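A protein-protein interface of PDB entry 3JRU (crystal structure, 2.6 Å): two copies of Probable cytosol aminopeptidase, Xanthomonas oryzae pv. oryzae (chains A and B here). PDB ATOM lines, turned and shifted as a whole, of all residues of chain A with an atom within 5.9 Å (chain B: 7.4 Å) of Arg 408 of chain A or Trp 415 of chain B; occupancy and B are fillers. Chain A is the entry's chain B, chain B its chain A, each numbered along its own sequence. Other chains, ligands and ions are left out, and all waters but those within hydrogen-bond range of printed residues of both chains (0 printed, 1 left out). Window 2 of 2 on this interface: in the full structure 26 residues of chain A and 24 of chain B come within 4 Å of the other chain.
The side-chain hydroxyl of Thr 384 of chain A is in hydrogen-bond range of the side-chain hydroxyl of Tyr 418 of chain B. The guanidinium group of Arg 408 of chain A lies within salt-bridge range of the side-chain carboxylate of Glu 417 of chain B (2.8 Å).
The backbone carbonyl oxygen of Gln 383 of chain A sits at hydrogen-bond distance from the guanidinium group of Arg 476 of chain A, at 2.8 Å. The backbone carbonyl oxygen of Arg 408 of chain A lies within hydrogen-bond range of the backbone NH of Ala 385 of chain A (3.1 Å). The backbone NH (N) of Trp 410 of chain A lies within hydrogen-bond range of the backbone carbonyl oxygen (O) of Ala 385 of chain A, at 2.7 Å. The backbone carbonyl oxygen of Phe 406 of chain A lies within hydrogen-bond range of the guanidinium group of Arg 408 of chain A (3.0 Å). O of Arg 408 of chain A sits at hydrogen-bond distance from NH2 of Arg 476 of chain A (3.5 Å).
Among the printed residues, merely in contact across the chains: Thr 384 of chain A with Trp 415 of chain B (3.2 Å), Gln 383 of chain A with Tyr 418 of chain B (3.3 Å), Trp 410 of chain A with Pro 413 of chain B (3.3 Å), Trp 410 of chain A with Trp 415 of chain B (3.6 Å), Arg 408 of chain A with Trp 415 of chain B (3.7 Å), Phe 406 of chain A with Glu 417 of chain B (3.8 Å), Trp 410 of chain A with Leu 412 of chain B (3.8 Å), Gln 383 of chain A with Glu 417 of chain B (3.8 Å) and Ala 409 of chain A with Trp 415 of chain B (3.9 Å).
Of chain B, only Trp 415 (3.7 Å) and Glu 417 (2.8 Å) come within 4 Å of Arg 408 of chain A. Trp 415 of chain B touches four residues of chain A. Printed residues of chain A within 4 Å of Glu 417 of chain B: Gln 383, Phe 406 and Arg 408. Printed residues of chain B within 4 Å of Gln 383 of chain A: Glu 417 (3.8 Å) and Tyr 418 (3.3 Å). Printed residues of chain A within 4 Å of Pro 413 of chain B: Trp 410 (3.3 Å). Of the printed residues of chain B, Ala 409 of chain A touches Trp 415. Of the printed residues of chain B, Phe 406 of chain A touches Glu 417.
Of the 13 printed residues of chain B, 5 touch a printed residue of chain A. Hydrophobic or aromatic side chains of chain B that line the printed part of chain A: Pro 413, Trp 415 and Tyr 418. Of the 13 printed residues of chain A, 6 touch a printed residue of chain B. Hydrophobic or aromatic side chains of chain A within 4 Å of the printed part of chain B: Phe 406 and Trp 410.
No position is printed for both chains. Of the 11 pairs that touch across the chains among the printed residues, none has its exchanged pair printed and touching as well.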
ATOM      1  N   GLN A 383       4.484 -16.007  22.879  1.00  0.00           N
ATOM      2  CA  GLN A 383       3.132 -16.029  22.345  1.00  0.00           C
ATOM      3  C   GLN A 383       2.220 -14.962  22.969  1.00  0.00           C
ATOM      4  O   GLN A 383       1.510 -14.279  22.240  1.00  0.00           O
ATOM      5  CB  GLN A 383       2.558 -17.446  22.417  1.00  0.00           C
ATOM      6  CG  GLN A 383       3.186 -18.356  21.361  1.00  0.00           C
ATOM      7  CD  GLN A 383       4.663 -18.865  21.663  1.00  0.00           C
ATOM      8  OE1 GLN A 383       5.312 -19.435  20.782  1.00  0.00           O
ATOM      9  NE2 GLN A 383       5.159 -18.679  22.892  1.00  0.00           N
ATOM     10  N   THR A 384       2.308 -14.766  24.296  1.00  0.00           N
ATOM     11  CA  THR A 384       1.263 -14.075  25.043  1.00  0.00           C
ATOM     12  C   THR A 384       1.832 -13.210  26.135  1.00  0.00           C
ATOM     13  O   THR A 384       2.737 -13.645  26.839  1.00  0.00           O
ATOM     14  CB  THR A 384       0.391 -15.115  25.775  1.00  0.00           C
ATOM     15  OG1 THR A 384       0.128 -16.223  24.895  1.00  0.00           O
ATOM     16  CG2 THR A 384      -0.888 -14.490  26.309  1.00  0.00           C
ATOM     17  N   ALA A 385       1.266 -12.025  26.326  1.00  0.00           N
ATOM     18  CA  ALA A 385       1.742 -11.113  27.367  1.00  0.00           C
ATOM     19  C   ALA A 385       1.143 -11.454  28.715  1.00  0.00           C
ATOM     20  O   ALA A 385       0.021 -11.957  28.783  1.00  0.00           O
ATOM     21  CB  ALA A 385       1.376  -9.672  27.001  1.00  0.00           C
ATOM     22  N   GLY A 402      -7.071  -7.831  23.347  1.00  0.00           N
ATOM     23  CA  GLY A 402      -6.019  -8.678  22.793  1.00  0.00           C
ATOM     24  C   GLY A 402      -6.561  -9.866  21.990  1.00  0.00           C
ATOM     25  O   GLY A 402      -6.057 -10.214  20.928  1.00  0.00           O
ATOM     26  N   GLU A 403      -7.609 -10.467  22.522  1.00  0.00           N
ATOM     27  CA  GLU A 403      -8.282 -11.599  21.915  1.00  0.00           C
ATOM     28  C   GLU A 403      -8.898 -11.188  20.553  1.00  0.00           C
ATOM     29  O   GLU A 403      -8.803 -11.931  19.549  1.00  0.00           O
ATOM     30  CB  GLU A 403      -9.320 -12.165  22.913  1.00  0.00           C
ATOM     31  CG  GLU A 403      -9.504 -13.713  22.828  1.00  0.00           C
ATOM     32  CD  GLU A 403      -8.286 -14.561  23.307  1.00  0.00           C
ATOM     33  OE1 GLU A 403      -7.938 -15.565  22.603  1.00  0.00           O
ATOM     34  OE2 GLU A 403      -7.682 -14.227  24.362  1.00  0.00           O
ATOM     35  N   PHE A 406      -6.139 -10.650  17.966  1.00  0.00           N
ATOM     36  CA  PHE A 406      -5.150 -11.754  18.069  1.00  0.00           C
ATOM     37  C   PHE A 406      -3.740 -11.308  18.465  1.00  0.00           C
ATOM     38  O   PHE A 406      -2.748 -11.719  17.851  1.00  0.00           O
ATOM     39  CB  PHE A 406      -5.106 -12.546  16.771  1.00  0.00           C
ATOM     40  CG  PHE A 406      -4.502 -13.944  16.909  1.00  0.00           C
ATOM     41  CD1 PHE A 406      -3.287 -14.256  16.273  1.00  0.00           C
ATOM     42  CD2 PHE A 406      -5.176 -14.952  17.626  1.00  0.00           C
ATOM     43  CE1 PHE A 406      -2.726 -15.529  16.379  1.00  0.00           C
ATOM     44  CE2 PHE A 406      -4.640 -16.217  17.745  1.00  0.00           C
ATOM     45  CZ  PHE A 406      -3.401 -16.518  17.120  1.00  0.00           C
ATOM     46  N   ASP A 407      -3.669 -10.428  19.455  1.00  0.00           N
ATOM     47  CA  ASP A 407      -2.438  -9.964  20.036  1.00  0.00           C
ATOM     48  C   ASP A 407      -2.693 -10.187  21.527  1.00  0.00           C
ATOM     49  O   ASP A 407      -2.984  -9.244  22.290  1.00  0.00           O
ATOM     50  CB  ASP A 407      -2.283  -8.487  19.707  1.00  0.00           C
ATOM     51  CG  ASP A 407      -1.015  -7.862  20.278  1.00  0.00           C
ATOM     52  OD1 ASP A 407      -0.101  -8.590  20.793  1.00  0.00           O
ATOM     53  OD2 ASP A 407      -0.943  -6.604  20.161  1.00  0.00           O
ATOM     54  N   ARG A 408      -2.573 -11.448  21.934  1.00  0.00           N
ATOM     55  CA  ARG A 408      -3.177 -11.971  23.136  1.00  0.00           C
ATOM     56  C   ARG A 408      -2.404 -11.651  24.444  1.00  0.00           C
ATOM     57  O   ARG A 408      -1.169 -11.496  24.455  1.00  0.00           O
ATOM     58  CB  ARG A 408      -3.381 -13.478  22.950  1.00  0.00           C
ATOM     59  CG  ARG A 408      -4.440 -13.906  21.839  1.00  0.00           C
ATOM     60  CD  ARG A 408      -4.172 -15.278  21.256  1.00  0.00           C
ATOM     61  NE  ARG A 408      -2.815 -15.606  20.641  1.00  0.00           N
ATOM     62  CZ  ARG A 408      -1.811 -14.774  20.174  1.00  0.00           C
ATOM     63  NH1 ARG A 408      -1.907 -13.434  20.183  1.00  0.00           N
ATOM     64  NH2 ARG A 408      -0.653 -15.299  19.664  1.00  0.00           N
ATOM     65  N   ALA A 409      -3.134 -11.490  25.541  1.00  0.00           N
ATOM     66  CA  ALA A 409      -2.497 -11.460  26.865  1.00  0.00           C
ATOM     67  C   ALA A 409      -3.111 -12.594  27.706  1.00  0.00           C
ATOM     68  O   ALA A 409      -4.046 -13.243  27.274  1.00  0.00           O
ATOM     69  CB  ALA A 409      -2.681 -10.139  27.512  1.00  0.00           C
ATOM     70  N   TRP A 410      -2.557 -12.878  28.867  1.00  0.00           N
ATOM     71  CA  TRP A 410      -3.140 -13.875  29.767  1.00  0.00           C
ATOM     72  C   TRP A 410      -2.954 -13.391  31.194  1.00  0.00           C
ATOM     73  O   TRP A 410      -1.858 -12.962  31.566  1.00  0.00           O
ATOM     74  CB  TRP A 410      -2.425 -15.188  29.585  1.00  0.00           C
ATOM     75  CG  TRP A 410      -2.954 -16.251  30.394  1.00  0.00           C
ATOM     76  CD1 TRP A 410      -2.472 -16.685  31.607  1.00  0.00           C
ATOM     77  CD2 TRP A 410      -4.082 -17.063  30.092  1.00  0.00           C
ATOM     78  NE1 TRP A 410      -3.233 -17.727  32.067  1.00  0.00           N
ATOM     79  CE2 TRP A 410      -4.227 -17.986  31.155  1.00  0.00           C
ATOM     80  CE3 TRP A 410      -4.977 -17.119  29.017  1.00  0.00           C
ATOM     81  CZ2 TRP A 410      -5.241 -18.963  31.174  1.00  0.00           C
ATOM     82  CZ3 TRP A 410      -6.003 -18.097  29.032  1.00  0.00           C
ATOM     83  CH2 TRP A 410      -6.124 -18.999  30.113  1.00  0.00           C
ATOM     84  N   VAL A 463       6.540 -10.891  24.049  1.00  0.00           N
ATOM     85  CA  VAL A 463       5.850 -10.503  22.836  1.00  0.00           C
ATOM     86  C   VAL A 463       6.494  -9.381  22.004  1.00  0.00           C
ATOM     87  O   VAL A 463       6.128  -9.179  20.838  1.00  0.00           O
ATOM     88  CB  VAL A 463       4.346 -10.149  23.132  1.00  0.00           C
ATOM     89  CG1 VAL A 463       3.666 -11.311  23.872  1.00  0.00           C
ATOM     90  CG2 VAL A 463       4.197  -8.813  23.908  1.00  0.00           C
ATOM     91  N   ARG A 476       4.256  -5.471  19.065  1.00  0.00           N
ATOM     92  CA  ARG A 476       3.268  -5.847  20.108  1.00  0.00           C
ATOM     93  C   ARG A 476       3.664  -5.134  21.404  1.00  0.00           C
ATOM     94  O   ARG A 476       4.853  -5.006  21.706  1.00  0.00           O
ATOM     95  CB  ARG A 476       3.199  -7.360  20.332  1.00  0.00           C
ATOM     96  CG  ARG A 476       2.822  -8.160  19.110  1.00  0.00           C
ATOM     97  CD  ARG A 476       2.947  -9.644  19.348  1.00  0.00           C
ATOM     98  NE  ARG A 476       1.941 -10.110  20.318  1.00  0.00           N
ATOM     99  CZ  ARG A 476       1.819 -11.358  20.761  1.00  0.00           C
ATOM    100  NH1 ARG A 476       2.602 -12.308  20.298  1.00  0.00           N
ATOM    101  NH2 ARG A 476       0.890 -11.646  21.666  1.00  0.00           N
ATOM    102  N   LEU A 480      -3.097  -4.733  20.616  1.00  0.00           N
ATOM    103  CA  LEU A 480      -3.962  -4.840  21.780  1.00  0.00           C
ATOM    104  C   LEU A 480      -4.380  -3.477  22.334  1.00  0.00           C
ATOM    105  O   LEU A 480      -5.585  -3.291  22.666  1.00  0.00           O
ATOM    106  CB  LEU A 480      -3.293  -5.669  22.880  1.00  0.00           C
ATOM    107  CG  LEU A 480      -4.088  -5.986  24.159  1.00  0.00           C
ATOM    108  CD1 LEU A 480      -3.484  -7.155  24.865  1.00  0.00           C
ATOM    109  CD2 LEU A 480      -4.119  -4.814  25.088  1.00  0.00           C
ATOM    110  N   SER B 389      -6.083 -27.321  30.654  1.00  0.00           N
ATOM    111  CA  SER B 389      -7.115 -28.199  30.079  1.00  0.00           C
ATOM    112  C   SER B 389      -7.726 -27.609  28.765  1.00  0.00           C
ATOM    113  O   SER B 389      -7.642 -26.405  28.524  1.00  0.00           O
ATOM    114  CB  SER B 389      -8.229 -28.427  31.105  1.00  0.00           C
ATOM    115  OG  SER B 389      -9.279 -29.198  30.541  1.00  0.00           O
ATOM    116  N   LYS B 390      -8.352 -28.450  27.937  1.00  0.00           N
ATOM    117  CA  LYS B 390      -9.043 -27.960  26.732  1.00  0.00           C
ATOM    118  C   LYS B 390     -10.547 -27.889  27.001  1.00  0.00           C
ATOM    119  O   LYS B 390     -11.333 -27.570  26.095  1.00  0.00           O
ATOM    120  CB  LYS B 390      -8.760 -28.860  25.522  1.00  0.00           C
ATOM    121  CG  LYS B 390      -7.297 -28.880  25.027  1.00  0.00           C
ATOM    122  CD  LYS B 390      -7.029 -27.655  24.072  1.00  0.00           C
ATOM    123  CE  LYS B 390      -5.684 -27.736  23.321  1.00  0.00           C
ATOM    124  NZ  LYS B 390      -5.503 -29.098  22.635  1.00  0.00           N
ATOM    125  N   LEU B 412      -3.277 -21.841  33.018  1.00  0.00           N
ATOM    126  CA  LEU B 412      -2.335 -21.409  32.008  1.00  0.00           C
ATOM    127  C   LEU B 412      -2.898 -21.912  30.699  1.00  0.00           C
ATOM    128  O   LEU B 412      -3.496 -22.979  30.652  1.00  0.00           O
ATOM    129  CB  LEU B 412      -0.968 -22.025  32.251  1.00  0.00           C
ATOM    130  CG  LEU B 412      -0.217 -21.563  33.502  1.00  0.00           C
ATOM    131  CD1 LEU B 412       1.102 -22.198  33.527  1.00  0.00           C
ATOM    132  CD2 LEU B 412      -0.043 -20.029  33.616  1.00  0.00           C
ATOM    133  N   PRO B 413      -2.746 -21.136  29.620  1.00  0.00           N
ATOM    134  CA  PRO B 413      -3.363 -21.483  28.323  1.00  0.00           C
ATOM    135  C   PRO B 413      -2.775 -22.728  27.664  1.00  0.00           C
ATOM    136  O   PRO B 413      -1.594 -22.997  27.822  1.00  0.00           O
ATOM    137  CB  PRO B 413      -3.005 -20.261  27.462  1.00  0.00           C
ATOM    138  CG  PRO B 413      -1.777 -19.717  28.106  1.00  0.00           C
ATOM    139  CD  PRO B 413      -1.993 -19.869  29.554  1.00  0.00           C
ATOM    140  N   LEU B 414      -3.569 -23.483  26.914  1.00  0.00           N
ATOM    141  CA  LEU B 414      -2.985 -24.533  26.077  1.00  0.00           C
ATOM    142  C   LEU B 414      -3.189 -24.246  24.590  1.00  0.00           C
ATOM    143  O   LEU B 414      -3.481 -25.166  23.816  1.00  0.00           O
ATOM    144  CB  LEU B 414      -3.552 -25.905  26.403  1.00  0.00           C
ATOM    145  CG  LEU B 414      -3.038 -26.763  27.548  1.00  0.00           C
ATOM    146  CD1 LEU B 414      -3.868 -28.044  27.538  1.00  0.00           C
ATOM    147  CD2 LEU B 414      -1.528 -27.084  27.548  1.00  0.00           C
ATOM    148  N   TRP B 415      -3.026 -22.988  24.181  1.00  0.00           N
ATOM    149  CA  TRP B 415      -3.360 -22.583  22.806  1.00  0.00           C
ATOM    150  C   TRP B 415      -2.564 -23.282  21.732  1.00  0.00           C
ATOM    151  O   TRP B 415      -1.459 -23.634  21.978  1.00  0.00           O
ATOM    152  CB  TRP B 415      -3.200 -21.084  22.651  1.00  0.00           C
ATOM    153  CG  TRP B 415      -4.097 -20.316  23.528  1.00  0.00           C
ATOM    154  CD1 TRP B 415      -5.285 -20.729  24.068  1.00  0.00           C
ATOM    155  CD2 TRP B 415      -3.880 -18.988  23.995  1.00  0.00           C
ATOM    156  NE1 TRP B 415      -5.821 -19.730  24.853  1.00  0.00           N
ATOM    157  CE2 TRP B 415      -4.981 -18.650  24.823  1.00  0.00           C
ATOM    158  CE3 TRP B 415      -2.853 -18.057  23.811  1.00  0.00           C
ATOM    159  CZ2 TRP B 415      -5.109 -17.411  25.426  1.00  0.00           C
ATOM    160  CZ3 TRP B 415      -2.985 -16.813  24.414  1.00  0.00           C
ATOM    161  CH2 TRP B 415      -4.104 -16.500  25.216  1.00  0.00           C
ATOM    162  N   ASP B 416      -3.127 -23.449  20.536  1.00  0.00           N
ATOM    163  CA  ASP B 416      -2.409 -24.111  19.422  1.00  0.00           C
ATOM    164  C   ASP B 416      -1.057 -23.508  19.036  1.00  0.00           C
ATOM    165  O   ASP B 416      -0.141 -24.244  18.620  1.00  0.00           O
ATOM    166  CB  ASP B 416      -3.256 -24.173  18.152  1.00  0.00           C
ATOM    167  CG  ASP B 416      -4.493 -25.034  18.309  1.00  0.00           C
ATOM    168  OD1 ASP B 416      -4.607 -25.775  19.335  1.00  0.00           O
ATOM    169  OD2 ASP B 416      -5.351 -24.947  17.382  1.00  0.00           O
ATOM    170  N   GLU B 417      -0.936 -22.185  19.156  1.00  0.00           N
ATOM    171  CA  GLU B 417       0.251 -21.482  18.634  1.00  0.00           C
ATOM    172  C   GLU B 417       1.466 -21.860  19.471  1.00  0.00           C
ATOM    173  O   GLU B 417       2.580 -21.499  19.145  1.00  0.00           O
ATOM    174  CB  GLU B 417       0.037 -19.954  18.554  1.00  0.00           C
ATOM    175  CG  GLU B 417      -0.708 -19.336  19.797  1.00  0.00           C
ATOM    176  CD  GLU B 417      -2.254 -19.269  19.645  1.00  0.00           C
ATOM    177  OE1 GLU B 417      -2.787 -20.078  18.831  1.00  0.00           O
ATOM    178  OE2 GLU B 417      -2.916 -18.385  20.336  1.00  0.00           O
ATOM    179  N   TYR B 418       1.230 -22.632  20.537  1.00  0.00           N
ATOM    180  CA  TYR B 418       2.313 -23.239  21.326  1.00  0.00           C
ATOM    181  C   TYR B 418       2.721 -24.624  20.836  1.00  0.00           C
ATOM    182  O   TYR B 418       3.737 -25.129  21.286  1.00  0.00           O
ATOM    183  CB  TYR B 418       1.927 -23.370  22.813  1.00  0.00           C
ATOM    184  CG  TYR B 418       1.871 -22.075  23.597  1.00  0.00           C
ATOM    185  CD1 TYR B 418       3.033 -21.472  24.084  1.00  0.00           C
ATOM    186  CD2 TYR B 418       0.655 -21.461  23.860  1.00  0.00           C
ATOM    187  CE1 TYR B 418       2.974 -20.286  24.825  1.00  0.00           C
ATOM    188  CE2 TYR B 418       0.583 -20.296  24.595  1.00  0.00           C
ATOM    189  CZ  TYR B 418       1.748 -19.704  25.092  1.00  0.00           C
ATOM    190  OH  TYR B 418       1.653 -18.509  25.813  1.00  0.00           O
ATOM    191  N   GLN B 419       1.935 -25.256  19.964  1.00  0.00           N
ATOM    192  CA  GLN B 419       2.154 -26.687  19.687  1.00  0.00           C
ATOM    193  C   GLN B 419       3.369 -26.894  18.858  1.00  0.00           C
ATOM    194  O   GLN B 419       4.001 -27.949  18.989  1.00  0.00           O
ATOM    195  CB  GLN B 419       0.969 -27.377  19.025  1.00  0.00           C
ATOM    196  CG  GLN B 419      -0.285 -27.419  19.919  1.00  0.00           C
ATOM    197  CD  GLN B 419      -0.233 -28.497  21.048  1.00  0.00           C
ATOM    198  OE1 GLN B 419       0.672 -29.373  21.074  1.00  0.00           O
ATOM    199  NE2 GLN B 419      -1.226 -28.445  21.964  1.00  0.00           N
ATOM    200  N   GLY B 420       3.721 -25.891  18.037  1.00  0.00           N
ATOM    201  CA  GLY B 420       4.795 -26.021  17.053  1.00  0.00           C
ATOM    202  C   GLY B 420       6.156 -26.177  17.698  1.00  0.00           C
ATOM    203  O   GLY B 420       7.083 -26.716  17.093  1.00  0.00           O
ATOM    204  N   ILE B 440       3.688 -24.741  29.799  1.00  0.00           N
ATOM    205  CA  ILE B 440       2.644 -24.823  28.766  1.00  0.00           C
ATOM    206  C   ILE B 440       2.940 -25.916  27.755  1.00  0.00           C
ATOM    207  O   ILE B 440       2.071 -26.721  27.410  1.00  0.00           O
ATOM    208  CB  ILE B 440       2.436 -23.454  28.024  1.00  0.00           C
ATOM    209  CG1 ILE B 440       1.831 -22.423  28.976  1.00  0.00           C
ATOM    210  CG2 ILE B 440       1.495 -23.607  26.839  1.00  0.00           C
ATOM    211  CD1 ILE B 440       1.863 -21.022  28.441  1.00  0.00           C
ATOM    212  N   CYS B 444       1.059 -29.031  26.677  1.00  0.00           N
ATOM    213  CA  CYS B 444       0.806 -29.385  25.294  1.00  0.00           C
ATOM    214  C   CYS B 444       1.271 -30.764  24.960  1.00  0.00           C
ATOM    215  O   CYS B 444       0.546 -31.487  24.272  1.00  0.00           O
ATOM    216  CB  CYS B 444       1.469 -28.402  24.347  1.00  0.00           C
ATOM    217  SG  CYS B 444       0.631 -26.792  24.397  1.00  0.00           S
